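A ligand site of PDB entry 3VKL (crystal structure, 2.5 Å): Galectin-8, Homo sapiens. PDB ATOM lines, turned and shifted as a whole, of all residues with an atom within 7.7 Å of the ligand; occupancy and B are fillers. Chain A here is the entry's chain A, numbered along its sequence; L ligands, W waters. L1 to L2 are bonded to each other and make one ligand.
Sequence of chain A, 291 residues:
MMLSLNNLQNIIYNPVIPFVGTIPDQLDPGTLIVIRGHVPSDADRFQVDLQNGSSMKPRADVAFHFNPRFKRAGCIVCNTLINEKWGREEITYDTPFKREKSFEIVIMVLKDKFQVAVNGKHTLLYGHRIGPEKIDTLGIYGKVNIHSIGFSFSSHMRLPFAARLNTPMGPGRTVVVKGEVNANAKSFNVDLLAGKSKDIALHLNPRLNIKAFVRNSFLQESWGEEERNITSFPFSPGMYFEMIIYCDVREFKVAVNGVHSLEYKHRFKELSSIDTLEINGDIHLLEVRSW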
ATOM      1  N   ARG A  45     -11.232   8.506 -11.259  1.00  0.00           N
ATOM      2  CA  ARG A  45     -10.314   8.158 -12.335  1.00  0.00           C
ATOM      3  C   ARG A  45     -10.998   7.627 -13.614  1.00  0.00           C
ATOM      4  O   ARG A  45     -12.071   7.043 -13.552  1.00  0.00           O
ATOM      5  CB  ARG A  45      -9.337   7.096 -11.803  1.00  0.00           C
ATOM      6  CG  ARG A  45      -8.831   6.118 -12.838  1.00  0.00           C
ATOM      7  CD  ARG A  45      -8.804   4.701 -12.282  1.00  0.00           C
ATOM      8  NE  ARG A  45      -7.512   4.326 -11.729  1.00  0.00           N
ATOM      9  CZ  ARG A  45      -6.530   3.693 -12.394  1.00  0.00           C
ATOM     10  NH1 ARG A  45      -5.408   3.417 -11.754  1.00  0.00           N
ATOM     11  NH2 ARG A  45      -6.665   3.346 -13.674  1.00  0.00           N
ATOM     12  N   GLN A  47      -9.862   6.339 -18.024  1.00  0.00           N
ATOM     13  CA  GLN A  47      -8.712   6.064 -18.874  1.00  0.00           C
ATOM     14  C   GLN A  47      -9.055   5.851 -20.334  1.00  0.00           C
ATOM     15  O   GLN A  47     -10.145   5.361 -20.649  1.00  0.00           O
ATOM     16  CB  GLN A  47      -7.968   4.814 -18.380  1.00  0.00           C
ATOM     17  CG  GLN A  47      -8.686   3.502 -18.676  1.00  0.00           C
ATOM     18  CD  GLN A  47      -8.212   2.349 -17.785  1.00  0.00           C
ATOM     19  OE1 GLN A  47      -8.320   2.408 -16.561  1.00  0.00           O
ATOM     20  NE2 GLN A  47      -7.704   1.290 -18.403  1.00  0.00           N
ATOM     21  N   ASP A  49      -7.482   3.948 -23.506  1.00  0.00           N
ATOM     22  CA  ASP A  49      -6.473   2.962 -23.873  1.00  0.00           C
ATOM     23  C   ASP A  49      -6.475   2.607 -25.345  1.00  0.00           C
ATOM     24  O   ASP A  49      -7.487   2.153 -25.882  1.00  0.00           O
ATOM     25  CB  ASP A  49      -6.707   1.664 -23.099  1.00  0.00           C
ATOM     26  CG  ASP A  49      -6.625   1.843 -21.597  1.00  0.00           C
ATOM     27  OD1 ASP A  49      -7.178   0.978 -20.868  1.00  0.00           O
ATOM     28  OD2 ASP A  49      -6.016   2.825 -21.131  1.00  0.00           O
ATOM     29  N   ARG A  59      -5.694 -10.291 -21.071  1.00  0.00           N
ATOM     30  CA  ARG A  59      -6.071  -8.910 -21.360  1.00  0.00           C
ATOM     31  C   ARG A  59      -5.221  -8.406 -22.506  1.00  0.00           C
ATOM     32  O   ARG A  59      -3.994  -8.523 -22.494  1.00  0.00           O
ATOM     33  CB  ARG A  59      -5.858  -8.026 -20.131  1.00  0.00           C
ATOM     34  CG  ARG A  59      -6.088  -6.559 -20.409  1.00  0.00           C
ATOM     35  CD  ARG A  59      -5.825  -5.729 -19.179  1.00  0.00           C
ATOM     36  NE  ARG A  59      -5.915  -4.311 -19.472  1.00  0.00           N
ATOM     37  CZ  ARG A  59      -5.671  -3.349 -18.593  1.00  0.00           C
ATOM     38  NH1 ARG A  59      -5.319  -3.669 -17.350  1.00  0.00           N
ATOM     39  NH2 ARG A  59      -5.788  -2.073 -18.938  1.00  0.00           N
ATOM     40  N   HIS A  65      -1.787   3.787 -22.593  1.00  0.00           N
ATOM     41  CA  HIS A  65      -2.742   3.946 -21.504  1.00  0.00           C
ATOM     42  C   HIS A  65      -2.675   5.421 -21.049  1.00  0.00           C
ATOM     43  O   HIS A  65      -1.638   5.875 -20.579  1.00  0.00           O
ATOM     44  CB  HIS A  65      -2.331   2.989 -20.366  1.00  0.00           C
ATOM     45  CG  HIS A  65      -3.120   3.143 -19.106  1.00  0.00           C
ATOM     46  ND1 HIS A  65      -4.434   2.727 -18.992  1.00  0.00           N
ATOM     47  CD2 HIS A  65      -2.759   3.581 -17.877  1.00  0.00           C
ATOM     48  CE1 HIS A  65      -4.834   2.890 -17.737  1.00  0.00           C
ATOM     49  NE2 HIS A  65      -3.843   3.411 -17.048  1.00  0.00           N
ATOM     50  N   PHE A  66      -3.771   6.151 -21.223  1.00  0.00           N
ATOM     51  CA  PHE A  66      -3.885   7.564 -20.836  1.00  0.00           C
ATOM     52  C   PHE A  66      -4.838   7.544 -19.640  1.00  0.00           C
ATOM     53  O   PHE A  66      -6.049   7.367 -19.807  1.00  0.00           O
ATOM     54  CB  PHE A  66      -4.529   8.351 -21.978  1.00  0.00           C
ATOM     55  CG  PHE A  66      -4.537   9.830 -21.773  1.00  0.00           C
ATOM     56  CD1 PHE A  66      -3.363  10.568 -21.839  1.00  0.00           C
ATOM     57  CD2 PHE A  66      -5.736  10.500 -21.539  1.00  0.00           C
ATOM     58  CE1 PHE A  66      -3.380  11.939 -21.691  1.00  0.00           C
ATOM     59  CE2 PHE A  66      -5.766  11.897 -21.380  1.00  0.00           C
ATOM     60  CZ  PHE A  66      -4.578  12.615 -21.463  1.00  0.00           C
ATOM     61  N   ASN A  67      -4.314   7.775 -18.451  1.00  0.00           N
ATOM     62  CA  ASN A  67      -5.144   7.652 -17.256  1.00  0.00           C
ATOM     63  C   ASN A  67      -5.191   8.852 -16.310  1.00  0.00           C
ATOM     64  O   ASN A  67      -4.379   8.995 -15.386  1.00  0.00           O
ATOM     65  CB  ASN A  67      -4.694   6.385 -16.520  1.00  0.00           C
ATOM     66  CG  ASN A  67      -5.391   6.186 -15.207  1.00  0.00           C
ATOM     67  OD1 ASN A  67      -4.857   5.527 -14.313  1.00  0.00           O
ATOM     68  ND2 ASN A  67      -6.596   6.743 -15.077  1.00  0.00           N
ATOM     69  N   ARG A  69      -6.123  10.933 -13.281  1.00  0.00           N
ATOM     70  CA  ARG A  69      -6.537  10.590 -11.940  1.00  0.00           C
ATOM     71  C   ARG A  69      -6.853  11.872 -11.186  1.00  0.00           C
ATOM     72  O   ARG A  69      -6.211  12.906 -11.376  1.00  0.00           O
ATOM     73  CB  ARG A  69      -5.442   9.791 -11.222  1.00  0.00           C
ATOM     74  CG  ARG A  69      -5.219   8.413 -11.822  1.00  0.00           C
ATOM     75  CD  ARG A  69      -4.194   7.612 -11.020  1.00  0.00           C
ATOM     76  NE  ARG A  69      -3.810   6.393 -11.736  1.00  0.00           N
ATOM     77  CZ  ARG A  69      -2.978   5.469 -11.245  1.00  0.00           C
ATOM     78  NH1 ARG A  69      -2.445   5.631 -10.038  1.00  0.00           N
ATOM     79  NH2 ARG A  69      -2.679   4.405 -11.969  1.00  0.00           N
ATOM     80  N   VAL A  77      -1.728   9.534 -15.533  1.00  0.00           N
ATOM     81  CA  VAL A  77      -0.786   8.426 -15.529  1.00  0.00           C
ATOM     82  C   VAL A  77      -0.773   7.715 -16.871  1.00  0.00           C
ATOM     83  O   VAL A  77      -1.819   7.307 -17.368  1.00  0.00           O
ATOM     84  CB  VAL A  77      -1.131   7.409 -14.419  1.00  0.00           C
ATOM     85  CG1 VAL A  77      -0.091   6.280 -14.411  1.00  0.00           C
ATOM     86  CG2 VAL A  77      -1.181   8.114 -13.049  1.00  0.00           C
ATOM     87  N   CYS A  78       0.420   7.590 -17.450  1.00  0.00           N
ATOM     88  CA  CYS A  78       0.580   6.931 -18.742  1.00  0.00           C
ATOM     89  C   CYS A  78       1.480   5.714 -18.629  1.00  0.00           C
ATOM     90  O   CYS A  78       2.467   5.716 -17.865  1.00  0.00           O
ATOM     91  CB  CYS A  78       1.152   7.898 -19.771  1.00  0.00           C
ATOM     92  SG  CYS A  78      -0.019   9.176 -20.231  1.00  0.00           S
ATOM     93  N   ASN A  79       1.153   4.677 -19.386  1.00  0.00           N
ATOM     94  CA  ASN A  79       1.938   3.463 -19.343  1.00  0.00           C
ATOM     95  C   ASN A  79       1.576   2.537 -20.495  1.00  0.00           C
ATOM     96  O   ASN A  79       0.660   2.812 -21.273  1.00  0.00           O
ATOM     97  CB  ASN A  79       1.705   2.732 -18.008  1.00  0.00           C
ATOM     98  CG  ASN A  79       2.908   1.933 -17.568  1.00  0.00           C
ATOM     99  OD1 ASN A  79       3.820   1.689 -18.346  1.00  0.00           O
ATOM    100  ND2 ASN A  79       2.894   1.508 -16.311  1.00  0.00           N
ATOM    101  N   THR A  80       2.296   1.428 -20.580  1.00  0.00           N
ATOM    102  CA  THR A  80       2.070   0.440 -21.627  1.00  0.00           C
ATOM    103  C   THR A  80       1.979  -0.922 -20.971  1.00  0.00           C
ATOM    104  O   THR A  80       2.668  -1.202 -19.994  1.00  0.00           O
ATOM    105  CB  THR A  80       3.237   0.422 -22.660  1.00  0.00           C
ATOM    106  OG1 THR A  80       3.241   1.647 -23.408  1.00  0.00           O
ATOM    107  CG2 THR A  80       3.093  -0.750 -23.613  1.00  0.00           C
ATOM    108  N   LEU A  81       1.084  -1.762 -21.483  1.00  0.00           N
ATOM    109  CA  LEU A  81       0.916  -3.109 -20.950  1.00  0.00           C
ATOM    110  C   LEU A  81       1.336  -4.144 -21.993  1.00  0.00           C
ATOM    111  O   LEU A  81       0.830  -4.147 -23.115  1.00  0.00           O
ATOM    112  CB  LEU A  81      -0.546  -3.329 -20.538  1.00  0.00           C
ATOM    113  CG  LEU A  81      -0.800  -4.605 -19.718  1.00  0.00           C
ATOM    114  CD1 LEU A  81      -0.279  -4.456 -18.292  1.00  0.00           C
ATOM    115  CD2 LEU A  81      -2.282  -4.878 -19.690  1.00  0.00           C
ATOM    116  N   TRP A  86       2.582  -4.177 -16.715  1.00  0.00           N
ATOM    117  CA  TRP A  86       2.828  -2.753 -16.897  1.00  0.00           C
ATOM    118  C   TRP A  86       4.295  -2.368 -17.018  1.00  0.00           C
ATOM    119  O   TRP A  86       5.170  -3.005 -16.452  1.00  0.00           O
ATOM    120  CB  TRP A  86       2.167  -1.955 -15.768  1.00  0.00           C
ATOM    121  CG  TRP A  86       0.674  -1.934 -15.847  1.00  0.00           C
ATOM    122  CD1 TRP A  86      -0.202  -2.534 -14.986  1.00  0.00           C
ATOM    123  CD2 TRP A  86      -0.139  -1.267 -16.837  1.00  0.00           C
ATOM    124  NE1 TRP A  86      -1.503  -2.291 -15.372  1.00  0.00           N
ATOM    125  CE2 TRP A  86      -1.493  -1.506 -16.504  1.00  0.00           C
ATOM    126  CE3 TRP A  86       0.154  -0.483 -17.969  1.00  0.00           C
ATOM    127  CZ2 TRP A  86      -2.557  -1.001 -17.258  1.00  0.00           C
ATOM    128  CZ3 TRP A  86      -0.902   0.024 -18.718  1.00  0.00           C
ATOM    129  CH2 TRP A  86      -2.240  -0.238 -18.361  1.00  0.00           C
ATOM    130  N   GLY A  87       4.533  -1.316 -17.783  1.00  0.00           N
ATOM    131  CA  GLY A  87       5.858  -0.786 -18.039  1.00  0.00           C
ATOM    132  C   GLY A  87       6.299   0.343 -17.111  1.00  0.00           C
ATOM    133  O   GLY A  87       5.882   0.405 -15.966  1.00  0.00           O
ATOM    134  N   ARG A  88       7.154   1.222 -17.627  1.00  0.00           N
ATOM    135  CA  ARG A  88       7.656   2.366 -16.858  1.00  0.00           C
ATOM    136  C   ARG A  88       6.502   3.365 -16.724  1.00  0.00           C
ATOM    137  O   ARG A  88       5.986   3.866 -17.719  1.00  0.00           O
ATOM    138  CB  ARG A  88       8.807   2.998 -17.658  1.00  0.00           C
ATOM    139  CG  ARG A  88       9.335   4.350 -17.165  1.00  0.00           C
ATOM    140  CD  ARG A  88       9.678   5.235 -18.354  1.00  0.00           C
ATOM    141  NE  ARG A  88      10.354   4.470 -19.401  1.00  0.00           N
ATOM    142  CZ  ARG A  88      10.379   4.793 -20.688  1.00  0.00           C
ATOM    143  NH1 ARG A  88       9.752   5.885 -21.125  1.00  0.00           N
ATOM    144  NH2 ARG A  88      11.037   4.024 -21.551  1.00  0.00           N
ATOM    145  N   GLU A  89       6.130   3.692 -15.496  1.00  0.00           N
ATOM    146  CA  GLU A  89       5.030   4.635 -15.302  1.00  0.00           C
ATOM    147  C   GLU A  89       5.502   6.067 -15.578  1.00  0.00           C
ATOM    148  O   GLU A  89       6.556   6.476 -15.093  1.00  0.00           O
ATOM    149  CB  GLU A  89       4.515   4.518 -13.871  1.00  0.00           C
ATOM    150  CG  GLU A  89       3.129   5.053 -13.679  1.00  0.00           C
ATOM    151  CD  GLU A  89       2.621   4.781 -12.290  1.00  0.00           C
ATOM    152  OE1 GLU A  89       3.199   5.352 -11.349  1.00  0.00           O
ATOM    153  OE2 GLU A  89       1.664   4.005 -12.148  1.00  0.00           O
ATOM    154  N   GLU A  90       4.696   6.839 -16.294  1.00  0.00           N
ATOM    155  CA  GLU A  90       5.021   8.229 -16.579  1.00  0.00           C
ATOM    156  C   GLU A  90       3.898   9.111 -16.102  1.00  0.00           C
ATOM    157  O   GLU A  90       2.807   9.095 -16.673  1.00  0.00           O
ATOM    158  CB  GLU A  90       5.302   8.418 -18.070  1.00  0.00           C
ATOM    159  CG  GLU A  90       6.683   7.886 -18.466  1.00  0.00           C
ATOM    160  CD  GLU A  90       6.895   7.696 -19.961  1.00  0.00           C
ATOM    161  OE1 GLU A  90       6.622   8.619 -20.760  1.00  0.00           O
ATOM    162  OE2 GLU A  90       7.359   6.612 -20.338  1.00  0.00           O
ATOM    163  N   ILE A  91       4.128   9.902 -15.068  1.00  0.00           N
ATOM    164  CA  ILE A  91       3.060  10.742 -14.562  1.00  0.00           C
ATOM    165  C   ILE A  91       3.200  12.199 -14.930  1.00  0.00           C
ATOM    166  O   ILE A  91       4.254  12.792 -14.751  1.00  0.00           O
ATOM    167  CB  ILE A  91       2.990  10.671 -13.024  1.00  0.00           C
ATOM    168  CG1 ILE A  91       2.769   9.224 -12.579  1.00  0.00           C
ATOM    169  CG2 ILE A  91       1.888  11.590 -12.517  1.00  0.00           C
ATOM    170  CD1 ILE A  91       2.697   9.055 -11.070  1.00  0.00           C
ATOM    171  N   ARG A 129       5.997   2.437 -27.557  1.00  0.00           N
ATOM    172  CA  ARG A 129       6.597   1.250 -26.961  1.00  0.00           C
ATOM    173  C   ARG A 129       6.154   0.022 -27.773  1.00  0.00           C
ATOM    174  O   ARG A 129       6.794  -1.031 -27.763  1.00  0.00           O
ATOM    175  CB  ARG A 129       6.188   1.109 -25.497  1.00  0.00           C
ATOM    176  CG  ARG A 129       6.692   2.229 -24.592  1.00  0.00           C
ATOM    177  CD  ARG A 129       6.263   1.962 -23.176  1.00  0.00           C
ATOM    178  NE  ARG A 129       6.597   3.036 -22.260  1.00  0.00           N
ATOM    179  CZ  ARG A 129       6.412   2.977 -20.945  1.00  0.00           C
ATOM    180  NH1 ARG A 129       5.900   1.879 -20.404  1.00  0.00           N
ATOM    181  NH2 ARG A 129       6.762   3.991 -20.176  1.00  0.00           N
HETATM  182  C1  LIG L   1       1.356   2.465  -8.194  1.00  0.00           C
HETATM  183  C2  LIG L   1       0.106   2.597  -9.063  1.00  0.00           C
HETATM  184  C3  LIG L   1      -0.074   1.408 -10.028  1.00  0.00           C
HETATM  185  C4  LIG L   1       0.175   0.055  -9.332  1.00  0.00           C
HETATM  186  C5  LIG L   1       0.254  -1.111 -10.309  1.00  0.00           C
HETATM  187  C6  LIG L   1       1.437   1.066  -7.575  1.00  0.00           C
HETATM  188  O1  LIG L   1       2.610   0.934  -6.844  1.00  0.00           O
HETATM  189  O2  LIG L   1       1.323   3.436  -7.159  1.00  0.00           O
HETATM  190  O3  LIG L   1       0.196   3.789  -9.822  1.00  0.00           O
HETATM  191  O4  LIG L   1      -1.416   1.433 -10.549  1.00  0.00           O
HETATM  192  O5  LIG L   1       1.435   0.081  -8.604  1.00  0.00           O
HETATM  193  O6  LIG L   1       1.341  -0.962 -11.217  1.00  0.00           O
HETATM  194  C1  LG2 L   2      -1.591   0.911 -11.816  1.00  0.00           C
HETATM  195  C2  LG2 L   2      -3.093   0.891 -12.176  1.00  0.00           C
HETATM  196  C3  LG2 L   2      -3.284   0.451 -13.626  1.00  0.00           C
HETATM  197  C4  LG2 L   2      -2.496   1.408 -14.506  1.00  0.00           C
HETATM  198  C5  LG2 L   2      -1.020   1.316 -14.108  1.00  0.00           C
HETATM  199  C6  LG2 L   2      -0.107   2.166 -14.948  1.00  0.00           C
HETATM  200  O1  LG2 L   2      -3.781  -0.008 -11.313  1.00  0.00           O
HETATM  201  O2  LG2 L   2      -4.660   0.475 -13.980  1.00  0.00           O
HETATM  202  O3  LG2 L   2      -2.977   2.729 -14.282  1.00  0.00           O
HETATM  203  O4  LG2 L   2      -0.875   1.745 -12.740  1.00  0.00           O
HETATM  204  O5  LG2 L   2       1.223   2.131 -14.442  1.00  0.00           O
HETATM  205  O   HOH W   1      -6.471  -0.646 -15.880  1.00  0.00           O
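NH1 of Arg 45 touches C2 of LG2 L2, at 3.5 Å.
CZ2 of Trp 86 touches C4 of LG2 L2, 3.7 Å away.
Seven residues have an atom within 4 Å of the ligand: Arg 45, His 65, Asn 67, Arg 69, Asn 79, Trp 86 and Glu 89.
Water W1 lies within hydrogen-bond range of O2 of LG2 L2 (2.9 Å), NE2 of Gln 47 (3.4 Å) and NH2 of Arg 59 (3.4 Å).
ND2 of Asn 79 lies within hydrogen-bond range of O5 of LG2 L2.
OE2 of Glu 89 lies within hydrogen-bond range of O3 of LIG L1 (2.8 Å).
The guanidinium group of Arg 69 is in hydrogen-bond range of an oxygen (O3) of LG2 L2 (2.9 Å).
NE2 of His 65 sits at hydrogen-bond distance from O3 of LG2 L2 (3.0 Å).
O3 of LG2 L2 lies within hydrogen-bond range of OD1 of Asn 67, at 3.4 Å.
The backbone carbonyl oxygen (O) of Asn 79 lies within hydrogen-bond range of the backbone NH (N) of His 65.
The side-chain amide oxygen (OD1) of Asn 79 lies close to the backbone NH (N) of Gly 87.
The side-chain amide oxygen (OD1) of Asn 79 lies close to the backbone carbonyl oxygen (O) of Arg 88 (3.1 Å).
OD1 of Asn 79 is in hydrogen-bond range of NH1 of Arg 129 (2.9 Å).
NE of Arg 69 is in hydrogen-bond range of OD1 of Asn 67 (2.9 Å).
The backbone carbonyl oxygen (O) of His 65 lies close to the side-chain sulfur (SG) of Cys 78, at 3.7 Å.
ND1 of His 65 is in hydrogen-bond range of OD2 of Asp 49, at 2.7 Å.
The guanidinium group (NH2) of Arg 45 is in hydrogen-bond range of the side-chain amide oxygen (OD1) of Asn 67, at 2.9 Å.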
